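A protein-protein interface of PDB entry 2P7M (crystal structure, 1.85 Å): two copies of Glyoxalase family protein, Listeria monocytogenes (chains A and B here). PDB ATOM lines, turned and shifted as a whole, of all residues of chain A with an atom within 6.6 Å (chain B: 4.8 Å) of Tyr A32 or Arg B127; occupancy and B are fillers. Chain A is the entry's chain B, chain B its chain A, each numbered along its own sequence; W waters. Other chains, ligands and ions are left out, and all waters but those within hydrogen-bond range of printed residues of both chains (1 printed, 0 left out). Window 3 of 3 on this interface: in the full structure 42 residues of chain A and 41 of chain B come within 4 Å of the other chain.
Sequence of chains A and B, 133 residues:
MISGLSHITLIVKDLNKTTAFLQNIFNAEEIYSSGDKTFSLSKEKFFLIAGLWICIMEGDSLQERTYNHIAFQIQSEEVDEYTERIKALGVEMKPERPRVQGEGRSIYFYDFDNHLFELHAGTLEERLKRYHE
The guanidinium group (NH2) of Arg B127 lies within salt-bridge range of the side-chain carboxylate (OE1) of Glu A44.
The guanidinium group (NH2) of Arg B127 is in hydrogen-bond range of the side-chain hydroxyl (OH) of Tyr A32 (3.3 Å).
N of Ile A31 sits at hydrogen-bond distance from O of Phe A46.
The backbone NH of Ser A34 is in hydrogen-bond range of the backbone carbonyl oxygen of Glu A44 (2.9 Å).
The backbone carbonyl oxygen (O) of Tyr A32 is in hydrogen-bond range of the backbone NH (N) of Phe A46 (2.9 Å).
Leu B124 touches Ile A31.
CD2 of Leu B128 touches O of Ile A31 (3.9 Å).
O of Ile A31 touches CE2 of Tyr B131 (3.6 Å).
CB of Tyr A32 touches CD2 of Leu B128, at 3.7 Å.
Tyr A32 touches Tyr B131.
CZ of Phe A46 touches NH1 of Arg B127, at 3.6 Å.
Trp A53 touches Leu B124.
Tyr A32 touches just these residues of chain B: Arg B127, Leu B128 and Tyr B131.
Of chain A, only Tyr A32, Glu A44 and Phe A46 come within 4 Å of Arg B127.
Of the printed residues of chain A, Leu B124 touches Ile A31 (3.9 Å) and Trp A53 (3.6 Å).
Printed residues of chain B within 4 Å of Phe A46: Arg B127 (3.6 Å).
Of the printed residues of chain A, Tyr B131 touches Ile A31 (3.6 Å) and Tyr A32 (3.5 Å).
Printed residues of chain B within 4 Å of Ile A31: Leu B124, Leu B128 and Tyr B131.
The nearest residue of chain B that does not touch Tyr A32 is Arg B130 (4.7 Å).
The nearest residue of chain A that does not touch Arg B127 is Trp A53 (4.7 Å).
The nearest printed residue of chain A that does not touch Leu B128 is Phe A46 (4.2 Å).
Printed residues of chain B that touch a printed residue of chain A: Leu B124, Arg B127, Leu B128 and Tyr B131.
Of the 12 printed residues of chain A, 5 touch a printed residue of chain B.
Hydrophobic or aromatic side chains of chain A within 4 Å of the printed part of chain B: Ile A31, Tyr A32, Phe A46 and Trp A53.
Among the printed residues, Asp or Glu carboxylates within 4 Å of a Lys or Arg side-chain nitrogen of the other chain: Glu A44 with Arg B127 (3.9 Å).
No position is printed for both chains.
Of the 9 pairs that touch across the chains among the printed residues, none has its exchanged pair printed and touching as well.
Water W1 bridges the side-chain hydroxyl (OH) of Tyr B131 (3.2 Å) and the backbone carbonyl oxygen (O) of Ser A33 (3.2 Å).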
ATOM      1  N   GLU A  29       2.684  33.850   0.945  1.00  0.00           N
ATOM      2  CA  GLU A  29       1.552  33.012   0.564  1.00  0.00           C
ATOM      3  C   GLU A  29       1.398  31.826   1.515  1.00  0.00           C
ATOM      4  O   GLU A  29       2.260  30.945   1.570  1.00  0.00           O
ATOM      5  CB  GLU A  29       1.751  32.484  -0.858  1.00  0.00           C
ATOM      6  CG  GLU A  29       0.588  31.662  -1.394  1.00  0.00           C
ATOM      7  CD  GLU A  29       0.974  30.812  -2.590  1.00  0.00           C
ATOM      8  OE1 GLU A  29       1.894  31.213  -3.337  1.00  0.00           O
ATOM      9  OE2 GLU A  29       0.351  29.748  -2.789  1.00  0.00           O
ATOM     10  N   GLU A  30       0.300  31.800   2.264  1.00  0.00           N
ATOM     11  CA  GLU A  30       0.045  30.697   3.189  1.00  0.00           C
ATOM     12  C   GLU A  30      -0.355  29.469   2.372  1.00  0.00           C
ATOM     13  O   GLU A  30      -1.269  29.538   1.555  1.00  0.00           O
ATOM     14  CB  GLU A  30      -1.073  31.073   4.168  1.00  0.00           C
ATOM     15  CG  GLU A  30      -1.556  29.932   5.049  1.00  0.00           C
ATOM     16  CD  GLU A  30      -2.528  30.395   6.127  1.00  0.00           C
ATOM     17  OE1 GLU A  30      -3.213  29.540   6.722  1.00  0.00           O
ATOM     18  OE2 GLU A  30      -2.597  31.611   6.387  1.00  0.00           O
ATOM     19  N   ILE A  31       0.333  28.353   2.598  1.00  0.00           N
ATOM     20  CA  ILE A  31       0.071  27.114   1.863  1.00  0.00           C
ATOM     21  C   ILE A  31      -0.246  25.944   2.785  1.00  0.00           C
ATOM     22  O   ILE A  31      -0.563  24.845   2.326  1.00  0.00           O
ATOM     23  CB  ILE A  31       1.292  26.704   1.015  1.00  0.00           C
ATOM     24  CG1 ILE A  31       2.524  26.596   1.925  1.00  0.00           C
ATOM     25  CG2 ILE A  31       1.523  27.713  -0.102  1.00  0.00           C
ATOM     26  CD1 ILE A  31       3.743  25.980   1.262  1.00  0.00           C
ATOM     27  N   TYR A  32      -0.159  26.174   4.087  1.00  0.00           N
ATOM     28  CA  TYR A  32      -0.412  25.113   5.046  1.00  0.00           C
ATOM     29  C   TYR A  32      -0.696  25.676   6.422  1.00  0.00           C
ATOM     30  O   TYR A  32      -0.110  26.680   6.832  1.00  0.00           O
ATOM     31  CB  TYR A  32       0.802  24.185   5.130  1.00  0.00           C
ATOM     32  CG  TYR A  32       0.669  23.054   6.129  1.00  0.00           C
ATOM     33  CD1 TYR A  32       0.096  21.835   5.761  1.00  0.00           C
ATOM     34  CD2 TYR A  32       1.133  23.195   7.442  1.00  0.00           C
ATOM     35  CE1 TYR A  32      -0.008  20.774   6.671  1.00  0.00           C
ATOM     36  CE2 TYR A  32       1.030  22.141   8.361  1.00  0.00           C
ATOM     37  CZ  TYR A  32       0.459  20.935   7.968  1.00  0.00           C
ATOM     38  OH  TYR A  32       0.347  19.894   8.868  1.00  0.00           O
ATOM     39  N   SER A  33      -1.588  25.006   7.136  1.00  0.00           N
ATOM     40  CA  SER A  33      -1.957  25.424   8.475  1.00  0.00           C
ATOM     41  C   SER A  33      -2.377  24.189   9.258  1.00  0.00           C
ATOM     42  O   SER A  33      -3.115  23.347   8.751  1.00  0.00           O
ATOM     43  CB  SER A  33      -3.112  26.427   8.407  1.00  0.00           C
ATOM     44  OG  SER A  33      -3.455  26.900   9.694  1.00  0.00           O
ATOM     45  N   SER A  34      -1.891  24.077  10.489  1.00  0.00           N
ATOM     46  CA  SER A  34      -2.237  22.948  11.337  1.00  0.00           C
ATOM     47  C   SER A  34      -2.272  23.398  12.791  1.00  0.00           C
ATOM     48  O   SER A  34      -1.789  24.478  13.132  1.00  0.00           O
ATOM     49  CB  SER A  34      -1.230  21.808  11.167  1.00  0.00           C
ATOM     50  OG  SER A  34       0.079  22.210  11.537  1.00  0.00           O
ATOM     51  N   GLY A  35      -2.854  22.563  13.643  1.00  0.00           N
ATOM     52  CA  GLY A  35      -2.946  22.902  15.048  1.00  0.00           C
ATOM     53  C   GLY A  35      -4.328  22.591  15.574  1.00  0.00           C
ATOM     54  O   GLY A  35      -5.324  22.734  14.866  1.00  0.00           O
ATOM     55  N   GLU A  44       0.706  25.920  13.718  1.00  0.00           N
ATOM     56  CA  GLU A  44       1.846  26.012  12.822  1.00  0.00           C
ATOM     57  C   GLU A  44       1.349  26.326  11.417  1.00  0.00           C
ATOM     58  O   GLU A  44       0.293  25.847  11.006  1.00  0.00           O
ATOM     59  CB  GLU A  44       2.614  24.693  12.829  1.00  0.00           C
ATOM     60  CG  GLU A  44       3.565  24.527  11.673  1.00  0.00           C
ATOM     61  CD  GLU A  44       4.412  23.282  11.808  1.00  0.00           C
ATOM     62  OE1 GLU A  44       3.843  22.197  12.064  1.00  0.00           O
ATOM     63  OE2 GLU A  44       5.646  23.393  11.652  1.00  0.00           O
ATOM     64  N   LYS A  45       2.096  27.151  10.694  1.00  0.00           N
ATOM     65  CA  LYS A  45       1.739  27.505   9.329  1.00  0.00           C
ATOM     66  C   LYS A  45       2.963  27.525   8.441  1.00  0.00           C
ATOM     67  O   LYS A  45       4.074  27.762   8.911  1.00  0.00           O
ATOM     68  CB  LYS A  45       1.078  28.882   9.259  1.00  0.00           C
ATOM     69  CG  LYS A  45      -0.394  28.905   9.615  1.00  0.00           C
ATOM     70  CD  LYS A  45      -0.966  30.297   9.344  1.00  0.00           C
ATOM     71  CE  LYS A  45      -2.450  30.385   9.670  1.00  0.00           C
ATOM     72  NZ  LYS A  45      -3.054  31.621   9.079  1.00  0.00           N
ATOM     73  N   PHE A  46       2.746  27.264   7.156  1.00  0.00           N
ATOM     74  CA  PHE A  46       3.814  27.294   6.169  1.00  0.00           C
ATOM     75  C   PHE A  46       3.475  28.412   5.200  1.00  0.00           C
ATOM     76  O   PHE A  46       2.314  28.582   4.827  1.00  0.00           O
ATOM     77  CB  PHE A  46       3.882  25.983   5.369  1.00  0.00           C
ATOM     78  CG  PHE A  46       4.246  24.767   6.180  1.00  0.00           C
ATOM     79  CD1 PHE A  46       4.180  23.500   5.602  1.00  0.00           C
ATOM     80  CD2 PHE A  46       4.642  24.876   7.513  1.00  0.00           C
ATOM     81  CE1 PHE A  46       4.499  22.358   6.337  1.00  0.00           C
ATOM     82  CE2 PHE A  46       4.963  23.745   8.256  1.00  0.00           C
ATOM     83  CZ  PHE A  46       4.890  22.483   7.667  1.00  0.00           C
ATOM     84  N   PHE A  47       4.480  29.179   4.800  1.00  0.00           N
ATOM     85  CA  PHE A  47       4.298  30.249   3.834  1.00  0.00           C
ATOM     86  C   PHE A  47       5.382  30.134   2.775  1.00  0.00           C
ATOM     87  O   PHE A  47       6.440  29.550   3.021  1.00  0.00           O
ATOM     88  CB  PHE A  47       4.455  31.627   4.472  1.00  0.00           C
ATOM     89  CG  PHE A  47       3.458  31.927   5.538  1.00  0.00           C
ATOM     90  CD1 PHE A  47       3.653  31.473   6.839  1.00  0.00           C
ATOM     91  CD2 PHE A  47       2.331  32.690   5.251  1.00  0.00           C
ATOM     92  CE1 PHE A  47       2.738  31.778   7.843  1.00  0.00           C
ATOM     93  CE2 PHE A  47       1.409  32.999   6.252  1.00  0.00           C
ATOM     94  CZ  PHE A  47       1.615  32.543   7.547  1.00  0.00           C
ATOM     95  N   TRP A  53      10.463  28.332   1.652  1.00  0.00           N
ATOM     96  CA  TRP A  53       9.553  27.709   2.597  1.00  0.00           C
ATOM     97  C   TRP A  53       9.814  28.272   3.998  1.00  0.00           C
ATOM     98  O   TRP A  53      10.886  28.068   4.572  1.00  0.00           O
ATOM     99  CB  TRP A  53       9.770  26.192   2.567  1.00  0.00           C
ATOM    100  CG  TRP A  53       8.902  25.366   3.494  1.00  0.00           C
ATOM    101  CD1 TRP A  53       7.801  25.782   4.195  1.00  0.00           C
ATOM    102  CD2 TRP A  53       9.051  23.965   3.780  1.00  0.00           C
ATOM    103  NE1 TRP A  53       7.259  24.726   4.899  1.00  0.00           N
ATOM    104  CE2 TRP A  53       8.006  23.602   4.662  1.00  0.00           C
ATOM    105  CE3 TRP A  53       9.968  22.982   3.375  1.00  0.00           C
ATOM    106  CZ2 TRP A  53       7.851  22.295   5.143  1.00  0.00           C
ATOM    107  CZ3 TRP A  53       9.814  21.682   3.857  1.00  0.00           C
ATOM    108  CH2 TRP A  53       8.762  21.353   4.730  1.00  0.00           C
ATOM    109  N   VAL B 100       5.113  13.567  12.113  1.00  0.00           N
ATOM    110  CA  VAL B 100       3.828  13.108  11.593  1.00  0.00           C
ATOM    111  C   VAL B 100       4.133  12.418  10.264  1.00  0.00           C
ATOM    112  O   VAL B 100       5.240  12.541   9.739  1.00  0.00           O
ATOM    113  CB  VAL B 100       2.849  14.275  11.327  1.00  0.00           C
ATOM    114  CG1 VAL B 100       2.408  14.903  12.640  1.00  0.00           C
ATOM    115  CG2 VAL B 100       3.505  15.314  10.429  1.00  0.00           C
ATOM    116  N   GLY B 102       4.587  11.747   6.480  1.00  0.00           N
ATOM    117  CA  GLY B 102       4.879  12.649   5.379  1.00  0.00           C
ATOM    118  C   GLY B 102       5.991  13.615   5.727  1.00  0.00           C
ATOM    119  O   GLY B 102       6.482  14.362   4.876  1.00  0.00           O
ATOM    120  N   GLU B 103       6.391  13.594   6.993  1.00  0.00           N
ATOM    121  CA  GLU B 103       7.449  14.465   7.485  1.00  0.00           C
ATOM    122  C   GLU B 103       8.755  13.676   7.505  1.00  0.00           C
ATOM    123  O   GLU B 103       8.929  12.768   8.318  1.00  0.00           O
ATOM    124  CB  GLU B 103       7.092  14.955   8.893  1.00  0.00           C
ATOM    125  CG  GLU B 103       8.096  15.905   9.512  1.00  0.00           C
ATOM    126  CD  GLU B 103       7.675  16.379  10.903  1.00  0.00           C
ATOM    127  OE1 GLU B 103       8.395  17.219  11.483  1.00  0.00           O
ATOM    128  OE2 GLU B 103       6.630  15.911  11.412  1.00  0.00           O
ATOM    129  N   THR B 123      10.621  16.553   2.170  1.00  0.00           N
ATOM    130  CA  THR B 123      10.236  17.523   1.152  1.00  0.00           C
ATOM    131  C   THR B 123       8.954  18.239   1.557  1.00  0.00           C
ATOM    132  O   THR B 123       8.199  17.758   2.405  1.00  0.00           O
ATOM    133  CB  THR B 123       9.961  16.849  -0.211  1.00  0.00           C
ATOM    134  OG1 THR B 123       8.842  15.962  -0.081  1.00  0.00           O
ATOM    135  CG2 THR B 123      11.182  16.074  -0.689  1.00  0.00           C
ATOM    136  N   LEU B 124       8.720  19.388   0.941  1.00  0.00           N
ATOM    137  CA  LEU B 124       7.518  20.167   1.208  1.00  0.00           C
ATOM    138  C   LEU B 124       6.323  19.441   0.595  1.00  0.00           C
ATOM    139  O   LEU B 124       5.262  19.335   1.210  1.00  0.00           O
ATOM    140  CB  LEU B 124       7.643  21.563   0.582  1.00  0.00           C
ATOM    141  CG  LEU B 124       6.383  22.442   0.532  1.00  0.00           C
ATOM    142  CD1 LEU B 124       5.829  22.655   1.947  1.00  0.00           C
ATOM    143  CD2 LEU B 124       6.713  23.784  -0.131  1.00  0.00           C
ATOM    144  N   GLU B 125       6.517  18.929  -0.619  1.00  0.00           N
ATOM    145  CA  GLU B 125       5.455  18.241  -1.341  1.00  0.00           C
ATOM    146  C   GLU B 125       4.903  17.049  -0.579  1.00  0.00           C
ATOM    147  O   GLU B 125       3.687  16.878  -0.474  1.00  0.00           O
ATOM    148  CB  GLU B 125       5.945  17.778  -2.714  1.00  0.00           C
ATOM    149  CG  GLU B 125       4.792  17.510  -3.679  1.00  0.00           C
ATOM    150  CD  GLU B 125       5.201  16.709  -4.898  1.00  0.00           C
ATOM    151  OE1 GLU B 125       6.280  16.977  -5.470  1.00  0.00           O
ATOM    152  OE2 GLU B 125       4.427  15.813  -5.290  1.00  0.00           O
ATOM    153  N   GLU B 126       5.796  16.218  -0.057  1.00  0.00           N
ATOM    154  CA  GLU B 126       5.365  15.050   0.695  1.00  0.00           C
ATOM    155  C   GLU B 126       4.533  15.522   1.877  1.00  0.00           C
ATOM    156  O   GLU B 126       3.472  14.965   2.172  1.00  0.00           O
ATOM    157  CB  GLU B 126       6.574  14.262   1.202  1.00  0.00           C
ATOM    158  CG  GLU B 126       6.207  12.972   1.920  1.00  0.00           C
ATOM    159  CD  GLU B 126       5.397  12.027   1.042  1.00  0.00           C
ATOM    160  OE1 GLU B 126       5.895  11.641  -0.042  1.00  0.00           O
ATOM    161  OE2 GLU B 126       4.263  11.673   1.435  1.00  0.00           O
ATOM    162  N   ARG B 127       5.017  16.568   2.535  1.00  0.00           N
ATOM    163  CA  ARG B 127       4.345  17.124   3.698  1.00  0.00           C
ATOM    164  C   ARG B 127       2.941  17.647   3.382  1.00  0.00           C
ATOM    165  O   ARG B 127       2.011  17.430   4.154  1.00  0.00           O
ATOM    166  CB  ARG B 127       5.209  18.237   4.305  1.00  0.00           C
ATOM    167  CG  ARG B 127       4.694  18.752   5.625  1.00  0.00           C
ATOM    168  CD  ARG B 127       4.449  17.605   6.588  1.00  0.00           C
ATOM    169  NE  ARG B 127       3.681  18.052   7.741  1.00  0.00           N
ATOM    170  CZ  ARG B 127       4.190  18.746   8.753  1.00  0.00           C
ATOM    171  NH1 ARG B 127       5.481  19.064   8.758  1.00  0.00           N
ATOM    172  NH2 ARG B 127       3.402  19.137   9.750  1.00  0.00           N
ATOM    173  N   LEU B 128       2.789  18.323   2.247  1.00  0.00           N
ATOM    174  CA  LEU B 128       1.494  18.869   1.844  1.00  0.00           C
ATOM    175  C   LEU B 128       0.580  17.814   1.215  1.00  0.00           C
ATOM    176  O   LEU B 128      -0.641  17.936   1.270  1.00  0.00           O
ATOM    177  CB  LEU B 128       1.684  20.004   0.830  1.00  0.00           C
ATOM    178  CG  LEU B 128       2.580  21.192   1.189  1.00  0.00           C
ATOM    179  CD1 LEU B 128       2.714  22.106  -0.024  1.00  0.00           C
ATOM    180  CD2 LEU B 128       1.993  21.947   2.374  1.00  0.00           C
ATOM    181  N   LYS B 129       1.169  16.784   0.616  1.00  0.00           N
ATOM    182  CA  LYS B 129       0.391  15.736  -0.040  1.00  0.00           C
ATOM    183  C   LYS B 129      -0.704  15.149   0.850  1.00  0.00           C
ATOM    184  O   LYS B 129      -1.883  15.164   0.488  1.00  0.00           O
ATOM    185  CB  LYS B 129       1.309  14.608  -0.517  1.00  0.00           C
ATOM    186  CG  LYS B 129       0.651  13.695  -1.540  1.00  0.00           C
ATOM    187  CD  LYS B 129       0.988  12.234  -1.297  1.00  0.00           C
ATOM    188  CE  LYS B 129       2.478  11.954  -1.410  1.00  0.00           C
ATOM    189  NZ  LYS B 129       2.757  10.524  -1.092  1.00  0.00           N
ATOM    190  N   ARG B 130      -0.311  14.617   2.002  1.00  0.00           N
ATOM    191  CA  ARG B 130      -1.265  14.033   2.937  1.00  0.00           C
ATOM    192  C   ARG B 130      -2.222  15.140   3.354  1.00  0.00           C
ATOM    193  O   ARG B 130      -3.440  15.007   3.247  1.00  0.00           O
ATOM    194  CB  ARG B 130      -0.535  13.496   4.170  1.00  0.00           C
ATOM    195  CG  ARG B 130      -1.415  12.702   5.122  1.00  0.00           C
ATOM    196  CD  ARG B 130      -0.767  12.573   6.494  1.00  0.00           C
ATOM    197  NE  ARG B 130      -0.720  13.858   7.190  1.00  0.00           N
ATOM    198  CZ  ARG B 130      -0.166  14.045   8.384  1.00  0.00           C
ATOM    199  NH1 ARG B 130       0.397  13.029   9.024  1.00  0.00           N
ATOM    200  NH2 ARG B 130      -0.179  15.250   8.940  1.00  0.00           N
ATOM    201  N   TYR B 131      -1.632  16.230   3.831  1.00  0.00           N
ATOM    202  CA  TYR B 131      -2.352  17.417   4.277  1.00  0.00           C
ATOM    203  C   TYR B 131      -3.671  17.639   3.541  1.00  0.00           C
ATOM    204  O   TYR B 131      -4.715  17.720   4.226  1.00  0.00           O
ATOM    205  CB  TYR B 131      -1.428  18.633   4.117  1.00  0.00           C
ATOM    206  CG  TYR B 131      -2.112  19.932   3.755  1.00  0.00           C
ATOM    207  CD1 TYR B 131      -3.034  20.523   4.613  1.00  0.00           C
ATOM    208  CD2 TYR B 131      -1.810  20.584   2.559  1.00  0.00           C
ATOM    209  CE1 TYR B 131      -3.638  21.730   4.291  1.00  0.00           C
ATOM    210  CE2 TYR B 131      -2.408  21.791   2.229  1.00  0.00           C
ATOM    211  CZ  TYR B 131      -3.320  22.361   3.098  1.00  0.00           C
ATOM    212  OH  TYR B 131      -3.910  23.562   2.776  1.00  0.00           O
HETATM  213  O   HOH W   1      -4.460  23.985   5.902  1.00  0.00           O
